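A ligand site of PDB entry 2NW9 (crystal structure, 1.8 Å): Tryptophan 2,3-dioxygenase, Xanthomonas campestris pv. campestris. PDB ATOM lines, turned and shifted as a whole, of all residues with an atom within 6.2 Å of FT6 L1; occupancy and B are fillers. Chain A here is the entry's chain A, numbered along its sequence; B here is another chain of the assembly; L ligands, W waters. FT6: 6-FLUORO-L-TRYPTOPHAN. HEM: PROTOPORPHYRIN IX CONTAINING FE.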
ATOM      1  N   PHE A  51      17.951   5.203  12.591  1.00  0.00           N
ATOM      2  CA  PHE A  51      18.637   4.847  13.824  1.00  0.00           C
ATOM      3  C   PHE A  51      20.143   4.797  13.617  1.00  0.00           C
ATOM      4  O   PHE A  51      20.899   5.396  14.379  1.00  0.00           O
ATOM      5  CB  PHE A  51      18.127   3.486  14.335  1.00  0.00           C
ATOM      6  CG  PHE A  51      18.635   3.131  15.702  1.00  0.00           C
ATOM      7  CD1 PHE A  51      18.072   3.695  16.840  1.00  0.00           C
ATOM      8  CD2 PHE A  51      19.653   2.195  15.851  1.00  0.00           C
ATOM      9  CE1 PHE A  51      18.533   3.348  18.121  1.00  0.00           C
ATOM     10  CE2 PHE A  51      20.117   1.835  17.111  1.00  0.00           C
ATOM     11  CZ  PHE A  51      19.557   2.412  18.246  1.00  0.00           C
ATOM     12  N   HIS A  55      23.235   7.880  14.690  1.00  0.00           N
ATOM     13  CA  HIS A  55      24.430   7.605  15.486  1.00  0.00           C
ATOM     14  C   HIS A  55      25.729   7.826  14.720  1.00  0.00           C
ATOM     15  O   HIS A  55      26.709   8.305  15.291  1.00  0.00           O
ATOM     16  CB  HIS A  55      24.428   6.167  16.007  1.00  0.00           C
ATOM     17  CG  HIS A  55      23.407   5.905  17.068  1.00  0.00           C
ATOM     18  ND1 HIS A  55      22.088   5.657  16.772  1.00  0.00           N
ATOM     19  CD2 HIS A  55      23.522   5.848  18.416  1.00  0.00           C
ATOM     20  CE1 HIS A  55      21.426   5.458  17.906  1.00  0.00           C
ATOM     21  NE2 HIS A  55      22.270   5.562  18.907  1.00  0.00           N
ATOM     22  N   TYR A 113      10.061   2.049  16.761  1.00  0.00           N
ATOM     23  CA  TYR A 113      11.243   1.529  17.430  1.00  0.00           C
ATOM     24  C   TYR A 113      11.112   0.080  17.875  1.00  0.00           C
ATOM     25  O   TYR A 113      12.009  -0.719  17.669  1.00  0.00           O
ATOM     26  CB  TYR A 113      11.584   2.384  18.650  1.00  0.00           C
ATOM     27  CG  TYR A 113      12.948   2.077  19.242  1.00  0.00           C
ATOM     28  CD1 TYR A 113      13.111   1.891  20.613  1.00  0.00           C
ATOM     29  CD2 TYR A 113      14.089   2.032  18.425  1.00  0.00           C
ATOM     30  CE1 TYR A 113      14.369   1.681  21.160  1.00  0.00           C
ATOM     31  CE2 TYR A 113      15.350   1.813  18.968  1.00  0.00           C
ATOM     32  CZ  TYR A 113      15.479   1.640  20.336  1.00  0.00           C
ATOM     33  OH  TYR A 113      16.745   1.470  20.872  1.00  0.00           O
ATOM     34  N   ARG A 117      14.123  -2.841  17.921  1.00  0.00           N
ATOM     35  CA  ARG A 117      14.972  -2.667  19.113  1.00  0.00           C
ATOM     36  C   ARG A 117      15.630  -3.968  19.543  1.00  0.00           C
ATOM     37  O   ARG A 117      16.749  -3.961  20.055  1.00  0.00           O
ATOM     38  CB  ARG A 117      14.161  -2.116  20.280  1.00  0.00           C
ATOM     39  CG  ARG A 117      15.025  -1.749  21.482  1.00  0.00           C
ATOM     40  CD  ARG A 117      14.233  -1.655  22.764  1.00  0.00           C
ATOM     41  NE  ARG A 117      15.021  -1.092  23.864  1.00  0.00           N
ATOM     42  CZ  ARG A 117      14.719  -1.236  25.151  1.00  0.00           C
ATOM     43  NH1 ARG A 117      15.498  -0.686  26.082  1.00  0.00           N
ATOM     44  NH2 ARG A 117      13.660  -1.948  25.512  1.00  0.00           N
ATOM     45  N   LEU A 120      19.305  -5.050  18.574  1.00  0.00           N
ATOM     46  CA  LEU A 120      20.433  -4.363  19.193  1.00  0.00           C
ATOM     47  C   LEU A 120      21.107  -5.184  20.286  1.00  0.00           C
ATOM     48  O   LEU A 120      22.284  -4.978  20.603  1.00  0.00           O
ATOM     49  CB  LEU A 120      19.980  -3.017  19.764  1.00  0.00           C
ATOM     50  CG  LEU A 120      19.300  -2.072  18.776  1.00  0.00           C
ATOM     51  CD1 LEU A 120      18.888  -0.793  19.490  1.00  0.00           C
ATOM     52  CD2 LEU A 120      20.244  -1.761  17.617  1.00  0.00           C
ATOM     53  N   SER A 123      23.947  -4.049  23.335  1.00  0.00           N
ATOM     54  CA  SER A 123      24.692  -2.855  22.950  1.00  0.00           C
ATOM     55  C   SER A 123      24.037  -1.570  23.455  1.00  0.00           C
ATOM     56  O   SER A 123      22.822  -1.533  23.677  1.00  0.00           O
ATOM     57  CB  SER A 123      24.843  -2.806  21.417  1.00  0.00           C
ATOM     58  OG  SER A 123      23.587  -2.712  20.769  1.00  0.00           O
ATOM     59  N   SER A 124      24.844  -0.534  23.650  1.00  0.00           N
ATOM     60  CA  SER A 124      24.325   0.740  24.124  1.00  0.00           C
ATOM     61  C   SER A 124      25.368   1.848  23.993  1.00  0.00           C
ATOM     62  O   SER A 124      26.535   1.587  23.705  1.00  0.00           O
ATOM     63  CB  SER A 124      23.903   0.655  25.585  1.00  0.00           C
ATOM     64  OG  SER A 124      25.037   0.675  26.440  1.00  0.00           O
ATOM     65  N   GLY A 125      24.936   3.084  24.241  1.00  0.00           N
ATOM     66  CA  GLY A 125      25.833   4.212  24.167  1.00  0.00           C
ATOM     67  C   GLY A 125      27.020   4.138  25.102  1.00  0.00           C
ATOM     68  O   GLY A 125      27.986   4.879  24.929  1.00  0.00           O
ATOM     69  N   GLN A 127      29.086   1.958  25.153  1.00  0.00           N
ATOM     70  CA  GLN A 127      30.166   1.428  24.343  1.00  0.00           C
ATOM     71  C   GLN A 127      30.689   2.403  23.295  1.00  0.00           C
ATOM     72  O   GLN A 127      31.415   2.002  22.385  1.00  0.00           O
ATOM     73  CB  GLN A 127      29.727   0.122  23.688  1.00  0.00           C
ATOM     74  CG  GLN A 127      29.262  -0.940  24.694  1.00  0.00           C
ATOM     75  CD  GLN A 127      28.683  -2.173  24.023  1.00  0.00           C
ATOM     76  OE1 GLN A 127      27.815  -2.076  23.148  1.00  0.00           O
ATOM     77  NE2 GLN A 127      29.146  -3.356  24.425  1.00  0.00           N
ATOM     78  N   ILE A 248      11.401   5.095  24.442  1.00  0.00           N
ATOM     79  CA  ILE A 248      11.243   3.891  25.263  1.00  0.00           C
ATOM     80  C   ILE A 248      10.578   4.148  26.606  1.00  0.00           C
ATOM     81  O   ILE A 248      10.304   3.214  27.360  1.00  0.00           O
ATOM     82  CB  ILE A 248      12.587   3.191  25.559  1.00  0.00           C
ATOM     83  CG1 ILE A 248      13.530   4.152  26.301  1.00  0.00           C
ATOM     84  CG2 ILE A 248      13.210   2.679  24.259  1.00  0.00           C
ATOM     85  CD1 ILE A 248      14.813   3.500  26.791  1.00  0.00           C
ATOM     86  N   ARG A 252      13.816  -0.214  31.125  1.00  0.00           N
ATOM     87  CA  ARG A 252      15.230  -0.296  31.449  1.00  0.00           C
ATOM     88  C   ARG A 252      16.005  -0.305  30.139  1.00  0.00           C
ATOM     89  O   ARG A 252      15.496  -0.765  29.117  1.00  0.00           O
ATOM     90  CB  ARG A 252      15.535  -1.560  32.258  1.00  0.00           C
ATOM     91  CG  ARG A 252      14.977  -1.525  33.679  1.00  0.00           C
ATOM     92  CD  ARG A 252      15.568  -2.624  34.557  1.00  0.00           C
ATOM     93  NE  ARG A 252      16.979  -2.383  34.862  1.00  0.00           N
ATOM     94  CZ  ARG A 252      17.414  -1.431  35.694  1.00  0.00           C
ATOM     95  NH1 ARG A 252      16.552  -0.624  36.298  1.00  0.00           N
ATOM     96  NH2 ARG A 252      18.711  -1.290  35.905  1.00  0.00           N
ATOM     97  N   GLY A 253      17.226   0.203  30.163  1.00  0.00           N
ATOM     98  CA  GLY A 253      18.026   0.252  28.951  1.00  0.00           C
ATOM     99  C   GLY A 253      18.717  -1.042  28.580  1.00  0.00           C
ATOM    100  O   GLY A 253      18.937  -1.909  29.426  1.00  0.00           O
ATOM    101  N   THR A 254      19.053  -1.183  27.303  1.00  0.00           N
ATOM    102  CA  THR A 254      19.730  -2.378  26.816  1.00  0.00           C
ATOM    103  C   THR A 254      21.114  -2.501  27.444  1.00  0.00           C
ATOM    104  O   THR A 254      21.690  -3.592  27.483  1.00  0.00           O
ATOM    105  CB  THR A 254      19.899  -2.316  25.292  1.00  0.00           C
ATOM    106  OG1 THR A 254      20.525  -1.079  24.929  1.00  0.00           O
ATOM    107  CG2 THR A 254      18.551  -2.415  24.603  1.00  0.00           C
ATOM    108  N   GLY A 255      21.638  -1.385  27.941  1.00  0.00           N
ATOM    109  CA  GLY A 255      22.951  -1.371  28.562  1.00  0.00           C
ATOM    110  C   GLY A 255      22.925  -1.811  30.020  1.00  0.00           C
ATOM    111  O   GLY A 255      23.978  -1.931  30.654  1.00  0.00           O
ATOM    112  N   THR B  23      28.003  -5.324  19.664  1.00  0.00           N
ATOM    113  CA  THR B  23      28.440  -4.130  20.372  1.00  0.00           C
ATOM    114  C   THR B  23      28.025  -2.886  19.609  1.00  0.00           C
ATOM    115  O   THR B  23      27.663  -2.945  18.436  1.00  0.00           O
ATOM    116  CB  THR B  23      29.966  -4.093  20.549  1.00  0.00           C
ATOM    117  OG1 THR B  23      30.596  -3.894  19.277  1.00  0.00           O
ATOM    118  CG2 THR B  23      30.462  -5.411  21.142  1.00  0.00           C
ATOM    119  N   TYR B  24      28.082  -1.747  20.290  1.00  0.00           N
ATOM    120  CA  TYR B  24      27.742  -0.462  19.708  1.00  0.00           C
ATOM    121  C   TYR B  24      28.579  -0.234  18.443  1.00  0.00           C
ATOM    122  O   TYR B  24      28.043   0.008  17.362  1.00  0.00           O
ATOM    123  CB  TYR B  24      28.024   0.625  20.752  1.00  0.00           C
ATOM    124  CG  TYR B  24      27.790   2.045  20.309  1.00  0.00           C
ATOM    125  CD1 TYR B  24      28.828   2.793  19.729  1.00  0.00           C
ATOM    126  CD2 TYR B  24      26.569   2.678  20.529  1.00  0.00           C
ATOM    127  CE1 TYR B  24      28.639   4.125  19.376  1.00  0.00           C
ATOM    128  CE2 TYR B  24      26.375   4.004  20.183  1.00  0.00           C
ATOM    129  CZ  TYR B  24      27.416   4.726  19.616  1.00  0.00           C
ATOM    130  OH  TYR B  24      27.230   6.057  19.293  1.00  0.00           O
ATOM    131  N   GLY B  25      29.903  -0.351  18.591  1.00  0.00           N
ATOM    132  CA  GLY B  25      30.798  -0.149  17.466  1.00  0.00           C
ATOM    133  C   GLY B  25      30.613  -1.167  16.357  1.00  0.00           C
ATOM    134  O   GLY B  25      30.756  -0.847  15.177  1.00  0.00           O
ATOM    135  N   TYR B  27      27.733  -2.880  15.626  1.00  0.00           N
ATOM    136  CA  TYR B  27      26.446  -2.634  14.968  1.00  0.00           C
ATOM    137  C   TYR B  27      26.554  -1.466  14.000  1.00  0.00           C
ATOM    138  O   TYR B  27      26.085  -1.536  12.852  1.00  0.00           O
ATOM    139  CB  TYR B  27      25.373  -2.325  16.021  1.00  0.00           C
ATOM    140  CG  TYR B  27      24.050  -1.901  15.423  1.00  0.00           C
ATOM    141  CD1 TYR B  27      23.279  -2.801  14.668  1.00  0.00           C
ATOM    142  CD2 TYR B  27      23.562  -0.608  15.594  1.00  0.00           C
ATOM    143  CE1 TYR B  27      22.074  -2.406  14.097  1.00  0.00           C
ATOM    144  CE2 TYR B  27      22.362  -0.205  15.033  1.00  0.00           C
ATOM    145  CZ  TYR B  27      21.620  -1.099  14.289  1.00  0.00           C
ATOM    146  OH  TYR B  27      20.423  -0.701  13.741  1.00  0.00           O
ATOM    147  N   LEU B  28      27.170  -0.384  14.460  1.00  0.00           N
ATOM    148  CA  LEU B  28      27.336   0.825  13.661  1.00  0.00           C
ATOM    149  C   LEU B  28      28.535   0.759  12.719  1.00  0.00           C
ATOM    150  O   LEU B  28      28.809   1.719  11.981  1.00  0.00           O
ATOM    151  CB  LEU B  28      27.487   2.027  14.595  1.00  0.00           C
ATOM    152  CG  LEU B  28      26.312   2.282  15.536  1.00  0.00           C
ATOM    153  CD1 LEU B  28      26.629   3.455  16.451  1.00  0.00           C
ATOM    154  CD2 LEU B  28      25.055   2.555  14.721  1.00  0.00           C
HETATM  155  N   FT6 L   1      20.241   1.743  24.989  1.00  0.00           N
HETATM  156  CA  FT6 L   1      19.230   1.771  23.890  1.00  0.00           C
HETATM  157  C   FT6 L   1      17.905   1.184  24.399  1.00  0.00           C
HETATM  158  OXT FT6 L   1      16.927   1.046  23.655  1.00  0.00           O
HETATM  159  CB  FT6 L   1      19.786   0.998  22.681  1.00  0.00           C
HETATM  160  CG  FT6 L   1      20.664   1.897  21.797  1.00  0.00           C
HETATM  161  CD2 FT6 L   1      21.686   1.483  20.961  1.00  0.00           C
HETATM  162  CD1 FT6 L   1      20.559   3.215  21.681  1.00  0.00           C
HETATM  163  NE1 FT6 L   1      21.479   3.676  20.799  1.00  0.00           N
HETATM  164  CE2 FT6 L   1      22.193   2.639  20.343  1.00  0.00           C
HETATM  165  CZ2 FT6 L   1      23.246   2.543  19.412  1.00  0.00           C
HETATM  166  CH2 FT6 L   1      23.773   1.265  19.124  1.00  0.00           C
HETATM  167  FAP FT6 L   1      24.780   1.137  18.236  1.00  0.00           F
HETATM  168  CZ3 FT6 L   1      23.273   0.105  19.731  1.00  0.00           C
HETATM  169  CE3 FT6 L   1      22.218   0.209  20.665  1.00  0.00           C
HETATM  170  O   FT6 L   1      17.808   0.843  25.586  1.00  0.00           O
HETATM  171  CHA HEM L   2      23.104   5.888  26.984  1.00  0.00           C
HETATM  172  CHB HEM L   2      18.688   5.055  24.971  1.00  0.00           C
HETATM  173  CHC HEM L   2      19.932   7.368  20.848  1.00  0.00           C
HETATM  174  CHD HEM L   2      24.325   8.156  22.844  1.00  0.00           C
HETATM  175  C1A HEM L   2      21.788   5.460  26.771  1.00  0.00           C
HETATM  176  C2A HEM L   2      20.949   4.691  27.783  1.00  0.00           C
HETATM  177  C3A HEM L   2      19.724   4.481  27.216  1.00  0.00           C
HETATM  178  C4A HEM L   2      19.741   5.059  25.882  1.00  0.00           C
HETATM  179  CMA HEM L   2      18.512   3.730  27.859  1.00  0.00           C
HETATM  180  CAA HEM L   2      21.444   4.256  29.202  1.00  0.00           C
HETATM  181  CBA HEM L   2      22.348   3.009  29.275  1.00  0.00           C
HETATM  182  CGA HEM L   2      21.464   1.814  29.020  1.00  0.00           C
HETATM  183  O1A HEM L   2      21.364   1.419  27.856  1.00  0.00           O
HETATM  184  O2A HEM L   2      20.886   1.296  29.982  1.00  0.00           O
HETATM  185  C1B HEM L   2      18.620   5.587  23.683  1.00  0.00           C
HETATM  186  C2B HEM L   2      17.445   5.526  22.785  1.00  0.00           C
HETATM  187  C3B HEM L   2      17.782   6.172  21.624  1.00  0.00           C
HETATM  188  C4B HEM L   2      19.176   6.645  21.784  1.00  0.00           C
HETATM  189  CMB HEM L   2      16.109   4.819  23.194  1.00  0.00           C
HETATM  190  CAB HEM L   2      16.931   6.409  20.329  1.00  0.00           C
HETATM  191  CBB HEM L   2      16.254   5.434  19.667  1.00  0.00           C
HETATM  192  C1C HEM L   2      21.255   7.805  20.988  1.00  0.00           C
HETATM  193  C2C HEM L   2      22.037   8.550  20.016  1.00  0.00           C
HETATM  194  C3C HEM L   2      23.265   8.769  20.564  1.00  0.00           C
HETATM  195  C4C HEM L   2      23.267   8.178  21.889  1.00  0.00           C
HETATM  196  CMC HEM L   2      21.550   9.009  18.604  1.00  0.00           C
HETATM  197  CAC HEM L   2      24.419   9.538  19.831  1.00  0.00           C
HETATM  198  CBC HEM L   2      25.471   8.756  19.373  1.00  0.00           C
HETATM  199  C1D HEM L   2      24.430   7.625  24.131  1.00  0.00           C
HETATM  200  C2D HEM L   2      25.603   7.690  25.017  1.00  0.00           C
HETATM  201  C3D HEM L   2      25.333   7.004  26.387  1.00  0.00           C
HETATM  202  C4D HEM L   2      23.932   6.571  26.120  1.00  0.00           C
HETATM  203  CMD HEM L   2      26.917   8.374  24.619  1.00  0.00           C
HETATM  204  CAD HEM L   2      26.342   6.922  27.505  1.00  0.00           C
HETATM  205  CBD HEM L   2      26.127   8.127  28.475  1.00  0.00           C
HETATM  206  CGD HEM L   2      26.709   8.137  29.640  1.00  0.00           C
HETATM  207  O1D HEM L   2      26.444   9.158  30.298  1.00  0.00           O
HETATM  208  O2D HEM L   2      27.516   7.048  29.969  1.00  0.00           O
HETATM  209  NA  HEM L   2      20.996   5.635  25.679  1.00  0.00           N
HETATM  210  NB  HEM L   2      19.611   6.276  23.017  1.00  0.00           N
HETATM  211  NC  HEM L   2      22.004   7.602  22.086  1.00  0.00           N
HETATM  212  ND  HEM L   2      23.473   6.936  24.852  1.00  0.00           N
HETATM  213 FE   HEM L   2      21.483   6.973  24.064  1.00  0.00          FE
HETATM  214  O   HOH W   1      22.320   3.560  24.180  1.00  0.00           O
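OG1 of Thr 254 lies within hydrogen-bond range of N of FT6 L1 (2.8 Å).
OH of Tyr 113 is in hydrogen-bond range of OXT of FT6 L1, 2.8 Å away.
The guanidinium group (NH1) of Arg 117 lies within salt-bridge range of an oxygen (O) of FT6 L1 (2.8 Å).
The backbone NH (N) of Thr 254 is in hydrogen-bond range of an oxygen (O) of FT6 L1, 2.9 Å away.
A ring nitrogen (NE2) of His 55 lies within hydrogen-bond range of a nitrogen (NE1) of FT6 L1, 2.8 Å away.
The backbone NH (N) of Gly 255 lies within hydrogen-bond range of an oxygen (O1A) of HEM L2 (2.8 Å).
A nitrogen (N) of FT6 L1 lies within hydrogen-bond range of an oxygen (O1A) of HEM L2.
N of Ser 124 sits at hydrogen-bond distance from OE1 of Gln 127 (3.4 Å).
ND1 of His 55 sits at hydrogen-bond distance from O of Phe 51, at 2.7 Å.
O of Leu 120 is in hydrogen-bond range of OG of Ser 123.
NH1 of Arg 117 sits at hydrogen-bond distance from O of Arg 252 (3.0 Å).
The side-chain hydroxyl of Thr 254 is in hydrogen-bond range of the backbone carbonyl oxygen of Ser 123 (2.7 Å).
The side-chain amide oxygen of Gln 127 lies within hydrogen-bond range of the backbone NH of Tyr 24 of chain B (2.9 Å).
Residues that only touch FT6 L1: Ser 123 (3.0 Å), Tyr 24 of chain B (3.3 Å), Leu 28 of chain B (3.3 Å), Phe 51 (3.4 Å), Tyr 27 of chain B (3.4 Å), Gly 253 (3.4 Å), Leu 120 (3.7 Å) and Ser 124 (3.9 Å).
Hydrophobic or aromatic side chains that line FT6 L1: Phe 51, His 55, Tyr 113, Leu 120, Tyr 24 of chain B, Tyr 27 of chain B and Leu 28 of chain B.
Within 4 Å of FT6 L1: Phe 51, His 55, Tyr 113, Arg 117, Leu 120, Ser 123, Ser 124, Gly 253, Thr 254, Tyr 24 of chain B, Tyr 27 of chain B and Leu 28 of chain B.
The nearest printed residue that does not touch FT6 L1 is Ile 248 (4.1 Å).
Water W1 lies within hydrogen-bond range of N of Gly 125 and N of FT6 L1.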
